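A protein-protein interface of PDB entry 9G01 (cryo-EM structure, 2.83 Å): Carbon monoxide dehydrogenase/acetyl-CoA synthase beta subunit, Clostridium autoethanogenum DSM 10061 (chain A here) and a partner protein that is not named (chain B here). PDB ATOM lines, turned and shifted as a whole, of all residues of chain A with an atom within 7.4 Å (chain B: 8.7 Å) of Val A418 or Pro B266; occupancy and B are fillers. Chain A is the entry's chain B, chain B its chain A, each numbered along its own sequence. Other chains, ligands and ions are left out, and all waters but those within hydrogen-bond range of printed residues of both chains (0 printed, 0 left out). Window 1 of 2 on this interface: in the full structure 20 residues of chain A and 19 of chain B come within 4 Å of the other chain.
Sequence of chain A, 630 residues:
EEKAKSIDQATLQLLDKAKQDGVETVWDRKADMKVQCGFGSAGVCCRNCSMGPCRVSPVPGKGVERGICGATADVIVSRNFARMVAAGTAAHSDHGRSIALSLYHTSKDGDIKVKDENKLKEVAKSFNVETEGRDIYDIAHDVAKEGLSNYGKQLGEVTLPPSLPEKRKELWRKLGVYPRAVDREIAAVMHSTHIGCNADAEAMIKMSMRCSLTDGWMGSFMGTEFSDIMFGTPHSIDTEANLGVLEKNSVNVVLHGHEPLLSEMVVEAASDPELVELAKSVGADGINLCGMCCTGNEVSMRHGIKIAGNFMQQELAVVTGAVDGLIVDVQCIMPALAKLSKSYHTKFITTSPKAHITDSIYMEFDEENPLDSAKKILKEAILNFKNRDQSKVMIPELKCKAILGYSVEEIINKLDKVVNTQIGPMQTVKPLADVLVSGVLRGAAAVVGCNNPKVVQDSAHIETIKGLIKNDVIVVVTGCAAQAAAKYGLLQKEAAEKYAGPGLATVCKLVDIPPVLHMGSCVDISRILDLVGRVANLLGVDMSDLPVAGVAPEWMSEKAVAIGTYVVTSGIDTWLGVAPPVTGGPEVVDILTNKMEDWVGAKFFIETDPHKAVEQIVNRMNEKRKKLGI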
ATOM      1  N   ASN A 413      21.260  -3.629 -17.215  1.00  0.00           N
ATOM      2  CA  ASN A 413      21.040  -3.753 -18.654  1.00  0.00           C
ATOM      3  C   ASN A 413      21.314  -5.179 -19.135  1.00  0.00           C
ATOM      4  O   ASN A 413      20.540  -5.734 -19.922  1.00  0.00           O
ATOM      5  CB  ASN A 413      21.929  -2.763 -19.424  1.00  0.00           C
ATOM      6  CG  ASN A 413      21.516  -1.300 -19.225  1.00  0.00           C
ATOM      7  OD1 ASN A 413      20.382  -1.019 -18.857  1.00  0.00           O
ATOM      8  ND2 ASN A 413      22.438  -0.370 -19.486  1.00  0.00           N
ATOM      9  N   LYS A 414      22.389  -5.802 -18.645  1.00  0.00           N
ATOM     10  CA  LYS A 414      22.678  -7.190 -19.014  1.00  0.00           C
ATOM     11  C   LYS A 414      21.598  -8.142 -18.509  1.00  0.00           C
ATOM     12  O   LYS A 414      21.177  -9.059 -19.225  1.00  0.00           O
ATOM     13  CB  LYS A 414      24.047  -7.615 -18.466  1.00  0.00           C
ATOM     14  CG  LYS A 414      25.238  -6.826 -19.048  1.00  0.00           C
ATOM     15  CD  LYS A 414      25.408  -7.076 -20.561  1.00  0.00           C
ATOM     16  CE  LYS A 414      25.779  -8.544 -20.834  1.00  0.00           C
ATOM     17  NZ  LYS A 414      26.030  -8.816 -22.290  1.00  0.00           N
ATOM     18  N   LEU A 415      21.123  -7.928 -17.284  1.00  0.00           N
ATOM     19  CA  LEU A 415      20.089  -8.784 -16.717  1.00  0.00           C
ATOM     20  C   LEU A 415      18.770  -8.666 -17.472  1.00  0.00           C
ATOM     21  O   LEU A 415      17.975  -9.611 -17.476  1.00  0.00           O
ATOM     22  CB  LEU A 415      19.895  -8.442 -15.239  1.00  0.00           C
ATOM     23  CG  LEU A 415      21.083  -8.771 -14.323  1.00  0.00           C
ATOM     24  CD1 LEU A 415      20.811  -8.187 -12.935  1.00  0.00           C
ATOM     25  CD2 LEU A 415      21.352 -10.280 -14.231  1.00  0.00           C
ATOM     26  N   ASP A 416      18.530  -7.534 -18.134  1.00  0.00           N
ATOM     27  CA  ASP A 416      17.310  -7.404 -18.928  1.00  0.00           C
ATOM     28  C   ASP A 416      17.205  -8.458 -20.028  1.00  0.00           C
ATOM     29  O   ASP A 416      16.096  -8.758 -20.478  1.00  0.00           O
ATOM     30  CB  ASP A 416      17.230  -6.015 -19.570  1.00  0.00           C
ATOM     31  CG  ASP A 416      16.724  -4.945 -18.615  1.00  0.00           C
ATOM     32  OD1 ASP A 416      16.567  -5.238 -17.410  1.00  0.00           O
ATOM     33  OD2 ASP A 416      16.481  -3.811 -19.066  1.00  0.00           O
ATOM     34  N   LYS A 417      18.331  -9.045 -20.441  1.00  0.00           N
ATOM     35  CA  LYS A 417      18.309 -10.045 -21.507  1.00  0.00           C
ATOM     36  C   LYS A 417      17.503 -11.275 -21.106  1.00  0.00           C
ATOM     37  O   LYS A 417      16.811 -11.865 -21.941  1.00  0.00           O
ATOM     38  CB  LYS A 417      19.748 -10.421 -21.877  1.00  0.00           C
ATOM     39  CG  LYS A 417      19.882 -11.642 -22.791  1.00  0.00           C
ATOM     40  CD  LYS A 417      21.354 -12.063 -22.886  1.00  0.00           C
ATOM     41  CE  LYS A 417      21.881 -11.941 -24.322  1.00  0.00           C
ATOM     42  NZ  LYS A 417      21.183 -12.914 -25.244  1.00  0.00           N
ATOM     43  N   VAL A 418      17.580 -11.682 -19.838  1.00  0.00           N
ATOM     44  CA  VAL A 418      16.936 -12.904 -19.369  1.00  0.00           C
ATOM     45  C   VAL A 418      15.553 -12.625 -18.761  1.00  0.00           C
ATOM     46  O   VAL A 418      15.011 -13.467 -18.051  1.00  0.00           O
ATOM     47  CB  VAL A 418      17.830 -13.678 -18.380  1.00  0.00           C
ATOM     48  CG1 VAL A 418      19.142 -14.132 -19.058  1.00  0.00           C
ATOM     49  CG2 VAL A 418      18.121 -12.851 -17.112  1.00  0.00           C
ATOM     50  N   VAL A 419      14.967 -11.460 -19.045  1.00  0.00           N
ATOM     51  CA  VAL A 419      13.637 -11.110 -18.552  1.00  0.00           C
ATOM     52  C   VAL A 419      12.629 -11.429 -19.650  1.00  0.00           C
ATOM     53  O   VAL A 419      12.722 -10.894 -20.763  1.00  0.00           O
ATOM     54  CB  VAL A 419      13.552  -9.625 -18.151  1.00  0.00           C
ATOM     55  CG1 VAL A 419      12.107  -9.255 -17.774  1.00  0.00           C
ATOM     56  CG2 VAL A 419      14.511  -9.298 -16.990  1.00  0.00           C
ATOM     57  N   ASN A 420      11.640 -12.262 -19.331  1.00  0.00           N
ATOM     58  CA  ASN A 420      10.549 -12.512 -20.267  1.00  0.00           C
ATOM     59  C   ASN A 420       9.742 -11.228 -20.431  1.00  0.00           C
ATOM     60  O   ASN A 420       9.269 -10.651 -19.445  1.00  0.00           O
ATOM     61  CB  ASN A 420       9.662 -13.666 -19.784  1.00  0.00           C
ATOM     62  CG  ASN A 420       8.694 -14.163 -20.875  1.00  0.00           C
ATOM     63  OD1 ASN A 420       7.735 -13.477 -21.209  1.00  0.00           O
ATOM     64  ND2 ASN A 420       8.954 -15.352 -21.435  1.00  0.00           N
ATOM     65  N   THR A 421       9.572 -10.786 -21.680  1.00  0.00           N
ATOM     66  CA  THR A 421       8.910  -9.509 -21.939  1.00  0.00           C
ATOM     67  C   THR A 421       7.470  -9.530 -21.448  1.00  0.00           C
ATOM     68  O   THR A 421       6.960  -8.513 -20.967  1.00  0.00           O
ATOM     69  CB  THR A 421       8.963  -9.170 -23.435  1.00  0.00           C
ATOM     70  OG1 THR A 421      10.316  -8.941 -23.849  1.00  0.00           O
ATOM     71  CG2 THR A 421       8.163  -7.921 -23.736  1.00  0.00           C
ATOM     72  N   MET A 426      11.208  -4.735 -16.281  1.00  0.00           N
ATOM     73  CA  MET A 426      12.522  -4.477 -16.841  1.00  0.00           C
ATOM     74  C   MET A 426      13.283  -3.507 -15.945  1.00  0.00           C
ATOM     75  O   MET A 426      12.710  -2.842 -15.076  1.00  0.00           O
ATOM     76  CB  MET A 426      12.402  -3.903 -18.265  1.00  0.00           C
ATOM     77  CG  MET A 426      11.799  -4.890 -19.300  1.00  0.00           C
ATOM     78  SD  MET A 426      12.884  -6.290 -19.647  1.00  0.00           S
ATOM     79  CE  MET A 426      11.923  -7.211 -20.840  1.00  0.00           C
ATOM     80  N   LYS A 430      15.981  -7.831 -10.392  1.00  0.00           N
ATOM     81  CA  LYS A 430      15.157  -9.004 -10.122  1.00  0.00           C
ATOM     82  C   LYS A 430      15.721 -10.305 -10.682  1.00  0.00           C
ATOM     83  O   LYS A 430      15.645 -11.320  -9.973  1.00  0.00           O
ATOM     84  CB  LYS A 430      13.735  -8.780 -10.640  1.00  0.00           C
ATOM     85  CG  LYS A 430      12.822  -9.973 -10.369  1.00  0.00           C
ATOM     86  CD  LYS A 430      11.383  -9.641 -10.749  1.00  0.00           C
ATOM     87  CE  LYS A 430      10.477 -10.871 -10.630  1.00  0.00           C
ATOM     88  NZ  LYS A 430      10.569 -11.475  -9.258  1.00  0.00           N
ATOM     89  N   PRO A 431      16.252 -10.378 -11.910  1.00  0.00           N
ATOM     90  CA  PRO A 431      16.854 -11.660 -12.344  1.00  0.00           C
ATOM     91  C   PRO A 431      17.974 -12.141 -11.426  1.00  0.00           C
ATOM     92  O   PRO A 431      18.070 -13.347 -11.150  1.00  0.00           O
ATOM     93  CB  PRO A 431      17.342 -11.366 -13.774  1.00  0.00           C
ATOM     94  CG  PRO A 431      16.463 -10.218 -14.258  1.00  0.00           C
ATOM     95  CD  PRO A 431      16.169  -9.391 -13.005  1.00  0.00           C
ATOM     96  N   LEU A 432      18.814 -11.227 -10.934  1.00  0.00           N
ATOM     97  CA  LEU A 432      19.876 -11.597 -10.000  1.00  0.00           C
ATOM     98  C   LEU A 432      19.298 -12.090  -8.678  1.00  0.00           C
ATOM     99  O   LEU A 432      19.744 -13.110  -8.133  1.00  0.00           O
ATOM    100  CB  LEU A 432      20.811 -10.403  -9.772  1.00  0.00           C
ATOM    101  CG  LEU A 432      21.924 -10.595  -8.722  1.00  0.00           C
ATOM    102  CD1 LEU A 432      22.876 -11.753  -9.107  1.00  0.00           C
ATOM    103  CD2 LEU A 432      22.701  -9.281  -8.516  1.00  0.00           C
ATOM    104  N   ALA A 433      18.275 -11.402  -8.172  1.00  0.00           N
ATOM    105  CA  ALA A 433      17.607 -11.855  -6.959  1.00  0.00           C
ATOM    106  C   ALA A 433      16.998 -13.235  -7.170  1.00  0.00           C
ATOM    107  O   ALA A 433      17.054 -14.084  -6.278  1.00  0.00           O
ATOM    108  CB  ALA A 433      16.541 -10.844  -6.526  1.00  0.00           C
ATOM    109  N   ASP A 434      16.437 -13.488  -8.356  1.00  0.00           N
ATOM    110  CA  ASP A 434      15.829 -14.785  -8.646  1.00  0.00           C
ATOM    111  C   ASP A 434      16.866 -15.897  -8.657  1.00  0.00           C
ATOM    112  O   ASP A 434      16.666 -16.945  -8.035  1.00  0.00           O
ATOM    113  CB  ASP A 434      15.107 -14.754  -9.996  1.00  0.00           C
ATOM    114  CG  ASP A 434      13.889 -13.856  -9.996  1.00  0.00           C
ATOM    115  OD1 ASP A 434      13.243 -13.741  -8.933  1.00  0.00           O
ATOM    116  OD2 ASP A 434      13.572 -13.266 -11.048  1.00  0.00           O
ATOM    117  N   VAL A 435      18.002 -15.677  -9.322  1.00  0.00           N
ATOM    118  CA  VAL A 435      19.013 -16.732  -9.379  1.00  0.00           C
ATOM    119  C   VAL A 435      19.597 -16.979  -7.991  1.00  0.00           C
ATOM    120  O   VAL A 435      19.887 -18.126  -7.631  1.00  0.00           O
ATOM    121  CB  VAL A 435      20.112 -16.427 -10.418  1.00  0.00           C
ATOM    122  CG1 VAL A 435      19.504 -16.301 -11.824  1.00  0.00           C
ATOM    123  CG2 VAL A 435      20.898 -15.178 -10.056  1.00  0.00           C
ATOM    124  N   LEU A 436      19.728 -15.928  -7.173  1.00  0.00           N
ATOM    125  CA  LEU A 436      20.219 -16.115  -5.805  1.00  0.00           C
ATOM    126  C   LEU A 436      19.203 -16.862  -4.946  1.00  0.00           C
ATOM    127  O   LEU A 436      19.576 -17.762  -4.186  1.00  0.00           O
ATOM    128  CB  LEU A 436      20.559 -14.764  -5.169  1.00  0.00           C
ATOM    129  CG  LEU A 436      21.831 -14.099  -5.717  1.00  0.00           C
ATOM    130  CD1 LEU A 436      21.980 -12.693  -5.136  1.00  0.00           C
ATOM    131  CD2 LEU A 436      23.102 -14.948  -5.441  1.00  0.00           C
ATOM    132  N   SER A 438      16.699 -18.894  -5.920  1.00  0.00           N
ATOM    133  CA  SER A 438      16.483 -20.268  -6.363  1.00  0.00           C
ATOM    134  C   SER A 438      17.643 -21.187  -5.989  1.00  0.00           C
ATOM    135  O   SER A 438      17.442 -22.400  -5.889  1.00  0.00           O
ATOM    136  CB  SER A 438      16.224 -20.322  -7.882  1.00  0.00           C
ATOM    137  OG  SER A 438      17.407 -20.059  -8.624  1.00  0.00           O
ATOM    138  N   VAL A 440      20.460 -21.385  -7.834  1.00  0.00           N
ATOM    139  CA  VAL A 440      21.318 -21.591  -8.999  1.00  0.00           C
ATOM    140  C   VAL A 440      22.664 -20.925  -8.754  1.00  0.00           C
ATOM    141  O   VAL A 440      23.720 -21.477  -9.086  1.00  0.00           O
ATOM    142  CB  VAL A 440      20.632 -21.079 -10.280  1.00  0.00           C
ATOM    143  CG1 VAL A 440      21.588 -21.137 -11.483  1.00  0.00           C
ATOM    144  CG2 VAL A 440      19.364 -21.911 -10.576  1.00  0.00           C
ATOM    145  N   THR A 506      26.062 -21.638 -16.254  1.00  0.00           N
ATOM    146  CA  THR A 506      24.765 -21.431 -16.892  1.00  0.00           C
ATOM    147  C   THR A 506      24.352 -19.965 -16.832  1.00  0.00           C
ATOM    148  O   THR A 506      23.913 -19.398 -17.841  1.00  0.00           O
ATOM    149  CB  THR A 506      23.703 -22.304 -16.218  1.00  0.00           C
ATOM    150  OG1 THR A 506      24.002 -23.690 -16.424  1.00  0.00           O
ATOM    151  CG2 THR A 506      22.311 -22.002 -16.777  1.00  0.00           C
ATOM    152  N   VAL A 507      24.524 -19.321 -15.677  1.00  0.00           N
ATOM    153  CA  VAL A 507      24.146 -17.913 -15.549  1.00  0.00           C
ATOM    154  C   VAL A 507      24.971 -17.055 -16.501  1.00  0.00           C
ATOM    155  O   VAL A 507      24.440 -16.168 -17.180  1.00  0.00           O
ATOM    156  CB  VAL A 507      24.287 -17.447 -14.087  1.00  0.00           C
ATOM    157  CG1 VAL A 507      24.143 -15.926 -13.978  1.00  0.00           C
ATOM    158  CG2 VAL A 507      23.243 -18.140 -13.202  1.00  0.00           C
ATOM    159  N   LYS A 509      26.418 -17.952 -19.304  1.00  0.00           N
ATOM    160  CA  LYS A 509      25.983 -18.186 -20.675  1.00  0.00           C
ATOM    161  C   LYS A 509      24.670 -17.470 -20.976  1.00  0.00           C
ATOM    162  O   LYS A 509      24.536 -16.821 -22.019  1.00  0.00           O
ATOM    163  CB  LYS A 509      25.863 -19.691 -20.919  1.00  0.00           C
ATOM    164  CG  LYS A 509      25.539 -20.041 -22.371  1.00  0.00           C
ATOM    165  CD  LYS A 509      25.616 -21.559 -22.614  1.00  0.00           C
ATOM    166  CE  LYS A 509      24.627 -22.336 -21.711  1.00  0.00           C
ATOM    167  NZ  LYS A 509      23.195 -21.903 -21.921  1.00  0.00           N
ATOM    168  N   LEU A 510      23.715 -17.518 -20.044  1.00  0.00           N
ATOM    169  CA  LEU A 510      22.415 -16.886 -20.271  1.00  0.00           C
ATOM    170  C   LEU A 510      22.522 -15.369 -20.342  1.00  0.00           C
ATOM    171  O   LEU A 510      21.911 -14.743 -21.214  1.00  0.00           O
ATOM    172  CB  LEU A 510      21.430 -17.291 -19.172  1.00  0.00           C
ATOM    173  CG  LEU A 510      20.970 -18.757 -19.189  1.00  0.00           C
ATOM    174  CD1 LEU A 510      20.096 -19.044 -17.975  1.00  0.00           C
ATOM    175  CD2 LEU A 510      20.221 -19.084 -20.486  1.00  0.00           C
ATOM    176  N   VAL A 511      23.293 -14.759 -19.438  1.00  0.00           N
ATOM    177  CA  VAL A 511      23.401 -13.303 -19.384  1.00  0.00           C
ATOM    178  C   VAL A 511      24.519 -12.776 -20.270  1.00  0.00           C
ATOM    179  O   VAL A 511      24.577 -11.563 -20.523  1.00  0.00           O
ATOM    180  CB  VAL A 511      23.605 -12.839 -17.924  1.00  0.00           C
ATOM    181  CG1 VAL A 511      23.513 -11.302 -17.798  1.00  0.00           C
ATOM    182  CG2 VAL A 511      22.588 -13.517 -16.995  1.00  0.00           C
ATOM    183  N   ASP A 512      25.406 -13.642 -20.760  1.00  0.00           N
ATOM    184  CA  ASP A 512      26.532 -13.242 -21.604  1.00  0.00           C
ATOM    185  C   ASP A 512      27.472 -12.285 -20.856  1.00  0.00           C
ATOM    186  O   ASP A 512      27.773 -11.182 -21.314  1.00  0.00           O
ATOM    187  CB  ASP A 512      26.039 -12.622 -22.914  1.00  0.00           C
ATOM    188  CG  ASP A 512      27.149 -12.465 -23.933  1.00  0.00           C
ATOM    189  OD1 ASP A 512      28.146 -13.212 -23.829  1.00  0.00           O
ATOM    190  OD2 ASP A 512      27.045 -11.593 -24.814  1.00  0.00           O
ATOM    191  N   ILE B 250      13.235 -29.243 -17.396  1.00  0.00           N
ATOM    192  CA  ILE B 250      14.318 -28.268 -17.490  1.00  0.00           C
ATOM    193  C   ILE B 250      15.619 -28.954 -17.885  1.00  0.00           C
ATOM    194  O   ILE B 250      16.382 -28.441 -18.710  1.00  0.00           O
ATOM    195  CB  ILE B 250      14.438 -27.491 -16.165  1.00  0.00           C
ATOM    196  CG1 ILE B 250      13.147 -26.676 -15.946  1.00  0.00           C
ATOM    197  CG2 ILE B 250      15.680 -26.591 -16.171  1.00  0.00           C
ATOM    198  CD1 ILE B 250      13.075 -25.940 -14.608  1.00  0.00           C
ATOM    199  N   PRO B 255      11.635 -25.081 -20.973  1.00  0.00           N
ATOM    200  CA  PRO B 255      11.244 -24.172 -19.885  1.00  0.00           C
ATOM    201  C   PRO B 255       9.888 -24.528 -19.300  1.00  0.00           C
ATOM    202  O   PRO B 255       8.975 -24.966 -20.003  1.00  0.00           O
ATOM    203  CB  PRO B 255      11.227 -22.785 -20.553  1.00  0.00           C
ATOM    204  CG  PRO B 255      11.011 -23.062 -22.037  1.00  0.00           C
ATOM    205  CD  PRO B 255      11.619 -24.430 -22.304  1.00  0.00           C
ATOM    206  N   VAL B 256       9.744 -24.285 -18.000  1.00  0.00           N
ATOM    207  CA  VAL B 256       8.530 -24.608 -17.263  1.00  0.00           C
ATOM    208  C   VAL B 256       7.884 -23.297 -16.834  1.00  0.00           C
ATOM    209  O   VAL B 256       8.499 -22.495 -16.120  1.00  0.00           O
ATOM    210  CB  VAL B 256       8.829 -25.515 -16.057  1.00  0.00           C
ATOM    211  CG1 VAL B 256       7.569 -25.741 -15.212  1.00  0.00           C
ATOM    212  CG2 VAL B 256       9.416 -26.855 -16.540  1.00  0.00           C
ATOM    213  N   PRO B 263      10.097 -20.541  -6.821  1.00  0.00           N
ATOM    214  CA  PRO B 263      11.394 -19.849  -6.932  1.00  0.00           C
ATOM    215  C   PRO B 263      11.829 -19.775  -8.386  1.00  0.00           C
ATOM    216  O   PRO B 263      12.311 -20.758  -8.955  1.00  0.00           O
ATOM    217  CB  PRO B 263      12.348 -20.711  -6.087  1.00  0.00           C
ATOM    218  CG  PRO B 263      11.446 -21.535  -5.180  1.00  0.00           C
ATOM    219  CD  PRO B 263      10.171 -21.748  -5.977  1.00  0.00           C
ATOM    220  N   GLU B 264      11.704 -18.591  -8.980  1.00  0.00           N
ATOM    221  CA  GLU B 264      11.894 -18.438 -10.415  1.00  0.00           C
ATOM    222  C   GLU B 264      13.360 -18.571 -10.806  1.00  0.00           C
ATOM    223  O   GLU B 264      14.261 -18.153 -10.071  1.00  0.00           O
ATOM    224  CB  GLU B 264      11.345 -17.090 -10.879  1.00  0.00           C
ATOM    225  CG  GLU B 264       9.828 -17.113 -11.099  1.00  0.00           C
ATOM    226  CD  GLU B 264       9.307 -15.766 -11.557  1.00  0.00           C
ATOM    227  OE1 GLU B 264       9.454 -14.789 -10.798  1.00  0.00           O
ATOM    228  OE2 GLU B 264       8.780 -15.676 -12.685  1.00  0.00           O
ATOM    229  N   VAL B 265      13.586 -19.172 -11.970  1.00  0.00           N
ATOM    230  CA  VAL B 265      14.891 -19.252 -12.606  1.00  0.00           C
ATOM    231  C   VAL B 265      14.760 -18.629 -13.996  1.00  0.00           C
ATOM    232  O   VAL B 265      14.003 -19.141 -14.827  1.00  0.00           O
ATOM    233  CB  VAL B 265      15.392 -20.706 -12.709  1.00  0.00           C
ATOM    234  CG1 VAL B 265      16.756 -20.754 -13.410  1.00  0.00           C
ATOM    235  CG2 VAL B 265      15.451 -21.351 -11.309  1.00  0.00           C
ATOM    236  N   PRO B 266      15.500 -17.558 -14.312  1.00  0.00           N
ATOM    237  CA  PRO B 266      15.305 -16.891 -15.610  1.00  0.00           C
ATOM    238  C   PRO B 266      15.465 -17.854 -16.778  1.00  0.00           C
ATOM    239  O   PRO B 266      16.358 -18.704 -16.801  1.00  0.00           O
ATOM    240  CB  PRO B 266      16.379 -15.792 -15.618  1.00  0.00           C
ATOM    241  CG  PRO B 266      16.620 -15.483 -14.151  1.00  0.00           C
ATOM    242  CD  PRO B 266      16.450 -16.831 -13.445  1.00  0.00           C
ATOM    243  N   THR B 267      14.534 -17.734 -17.731  1.00  0.00           N
ATOM    244  CA  THR B 267      14.467 -18.514 -18.962  1.00  0.00           C
ATOM    245  C   THR B 267      14.138 -19.994 -18.729  1.00  0.00           C
ATOM    246  O   THR B 267      13.899 -20.722 -19.695  1.00  0.00           O
ATOM    247  CB  THR B 267      15.778 -18.406 -19.773  1.00  0.00           C
ATOM    248  OG1 THR B 267      16.806 -19.228 -19.204  1.00  0.00           O
ATOM    249  CG2 THR B 267      16.275 -16.959 -19.847  1.00  0.00           C
ATOM    250  N   LEU B 268      14.052 -20.442 -17.475  1.00  0.00           N
ATOM    251  CA  LEU B 268      13.825 -21.855 -17.184  1.00  0.00           C
ATOM    252  C   LEU B 268      12.563 -22.112 -16.373  1.00  0.00           C
ATOM    253  O   LEU B 268      11.760 -22.972 -16.746  1.00  0.00           O
ATOM    254  CB  LEU B 268      15.052 -22.451 -16.461  1.00  0.00           C
ATOM    255  CG  LEU B 268      16.363 -22.418 -17.268  1.00  0.00           C
ATOM    256  CD1 LEU B 268      17.502 -23.076 -16.476  1.00  0.00           C
ATOM    257  CD2 LEU B 268      16.194 -23.097 -18.630  1.00  0.00           C
ATOM    258  N   LEU B 269      12.358 -21.390 -15.275  1.00  0.00           N
ATOM    259  CA  LEU B 269      11.196 -21.574 -14.414  1.00  0.00           C
ATOM    260  C   LEU B 269      10.577 -20.198 -14.209  1.00  0.00           C
ATOM    261  O   LEU B 269      11.200 -19.318 -13.605  1.00  0.00           O
ATOM    262  CB  LEU B 269      11.600 -22.228 -13.092  1.00  0.00           C
ATOM    263  CG  LEU B 269      10.450 -22.575 -12.144  1.00  0.00           C
ATOM    264  CD1 LEU B 269       9.435 -23.502 -12.814  1.00  0.00           C
ATOM    265  CD2 LEU B 269      11.015 -23.215 -10.877  1.00  0.00           C
ATOM    266  N   LEU B 270       9.367 -20.008 -14.732  1.00  0.00           N
ATOM    267  CA  LEU B 270       8.732 -18.701 -14.793  1.00  0.00           C
ATOM    268  C   LEU B 270       7.311 -18.769 -14.256  1.00  0.00           C
ATOM    269  O   LEU B 270       6.577 -19.722 -14.530  1.00  0.00           O
ATOM    270  CB  LEU B 270       8.708 -18.167 -16.236  1.00  0.00           C
ATOM    271  CG  LEU B 270      10.061 -18.088 -16.962  1.00  0.00           C
ATOM    272  CD1 LEU B 270       9.835 -17.598 -18.394  1.00  0.00           C
ATOM    273  CD2 LEU B 270      11.066 -17.187 -16.233  1.00  0.00           C
ATOM    274  N   THR B 271       6.917 -17.727 -13.531  1.00  0.00           N
ATOM    275  CA  THR B 271       5.566 -17.599 -13.010  1.00  0.00           C
ATOM    276  C   THR B 271       4.815 -16.572 -13.846  1.00  0.00           C
ATOM    277  O   THR B 271       5.302 -15.455 -14.046  1.00  0.00           O
ATOM    278  CB  THR B 271       5.572 -17.161 -11.537  1.00  0.00           C
ATOM    279  OG1 THR B 271       6.082 -18.209 -10.699  1.00  0.00           O
ATOM    280  CG2 THR B 271       4.158 -16.791 -11.067  1.00  0.00           C
ATOM    281  N   GLU B 284       7.376 -16.795 -26.195  1.00  0.00           N
ATOM    282  CA  GLU B 284       8.613 -16.049 -26.005  1.00  0.00           C
ATOM    283  C   GLU B 284       9.656 -16.868 -25.255  1.00  0.00           C
ATOM    284  O   GLU B 284      10.839 -16.844 -25.611  1.00  0.00           O
ATOM    285  CB  GLU B 284       8.342 -14.738 -25.269  1.00  0.00           C
ATOM    286  CG  GLU B 284       9.629 -13.945 -25.027  1.00  0.00           C
ATOM    287  CD  GLU B 284       9.402 -12.675 -24.232  1.00  0.00           C
ATOM    288  OE1 GLU B 284       8.239 -12.247 -24.115  1.00  0.00           O
ATOM    289  OE2 GLU B 284      10.386 -12.106 -23.713  1.00  0.00           O
ATOM    290  N   ALA B 285       9.242 -17.604 -24.219  1.00  0.00           N
ATOM    291  CA  ALA B 285      10.196 -18.356 -23.406  1.00  0.00           C
ATOM    292  C   ALA B 285      10.829 -19.488 -24.196  1.00  0.00           C
ATOM    293  O   ALA B 285      12.002 -19.808 -23.985  1.00  0.00           O
ATOM    294  CB  ALA B 285       9.528 -18.897 -22.138  1.00  0.00           C
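Along chain A the printed residues that touch a printed residue of chain B span positions 418 to 510. Of the 14 printed residues of chain B, 7 touch a printed residue of chain A. Printed residues of chain B that touch a printed residue of chain A: Glu B264, Val B265, Pro B266, Thr B267, Leu B270, Glu B284 and Ala B285. Among the printed residues, 15 pairs touch across the chains.
CB of Pro B266 touches O of Val A418, at 3.6 Å. CB of Val A418 touches CG2 of Thr B267 (3.9 Å). Val A419 touches Glu B284 (O to OE2, 3.95 Å). Leu B270 touches Asn A420 (CD1 to ND2, 3.9 Å). Asn A420 touches Ala B285 (ND2 to N, 3.6 Å). Pro A431 touches Pro B266. Val A435 touches Pro B266 (CG1 to CD, 3.5 Å). CG2 of Val B265 touches OG of Ser A438, 3.6 Å away. Leu A510 touches Pro B266 (CD1 to O, 3.9 Å). CD1 of Leu A510 touches OG1 of Thr B267 (3.5 Å).
Of chain B, only Pro B266 and Thr B267 come within 4 Å of Val A418. Of the printed residues of chain B, Thr A421 touches Glu B284 (2.6 Å). Of the printed residues of chain A, Glu B264 touches Lys A430, Asp A434 and Ser A438. Printed residues of chain A within 4 Å of Leu B270: Asn A420. Of the printed residues of chain B, Lys A430 touches Glu B264 (3.8 Å). Of the printed residues of chain B, Val A435 touches Pro B266. Val A511 touches none of the printed residues of chain B. Val A440 touches none of the printed residues of chain B. The nearest residue of chain B that does not touch Val A418 is Leu B270 (5.7 Å). The nearest residue of chain A that does not touch Pro B266 is Asp A434 (4.2 Å).
OE1 of Glu B264 is in salt-bridge range of NZ of Lys A430, 3.8 Å away. OE1 of Glu B284 lies close to OD1 of Asn A420, 3.2 Å away. The side-chain carboxylate (OE2) of Glu B284 is in hydrogen-bond range of the backbone NH (N) of Thr A421, at 2.6 Å. The backbone carbonyl oxygen (O) of Asp A434 lies close to the backbone carbonyl oxygen (O) of Glu B264, at 3.4 Å.
The backbone NH (N) of Leu B270 sits at hydrogen-bond distance from the backbone carbonyl oxygen (O) of Val B256, at 3.0 Å. The backbone NH (N) of Thr B271 is in hydrogen-bond range of the side-chain carboxylate (OE2) of Glu B264. The side-chain amino group (NZ) of Lys A430 is in salt-bridge range of the side-chain carboxylate (OD1) of Asp A434 (3.5 Å). O of Asp A434 sits at hydrogen-bond distance from OG of Ser A438 (3.3 Å). The backbone carbonyl oxygen (O) of Val A435 lies within hydrogen-bond range of the backbone NH (N) of Val A440, 3.3 Å away. The side-chain hydroxyl (OG) of Ser A438 lies close to the backbone NH (N) of Val A440 (3.4 Å).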
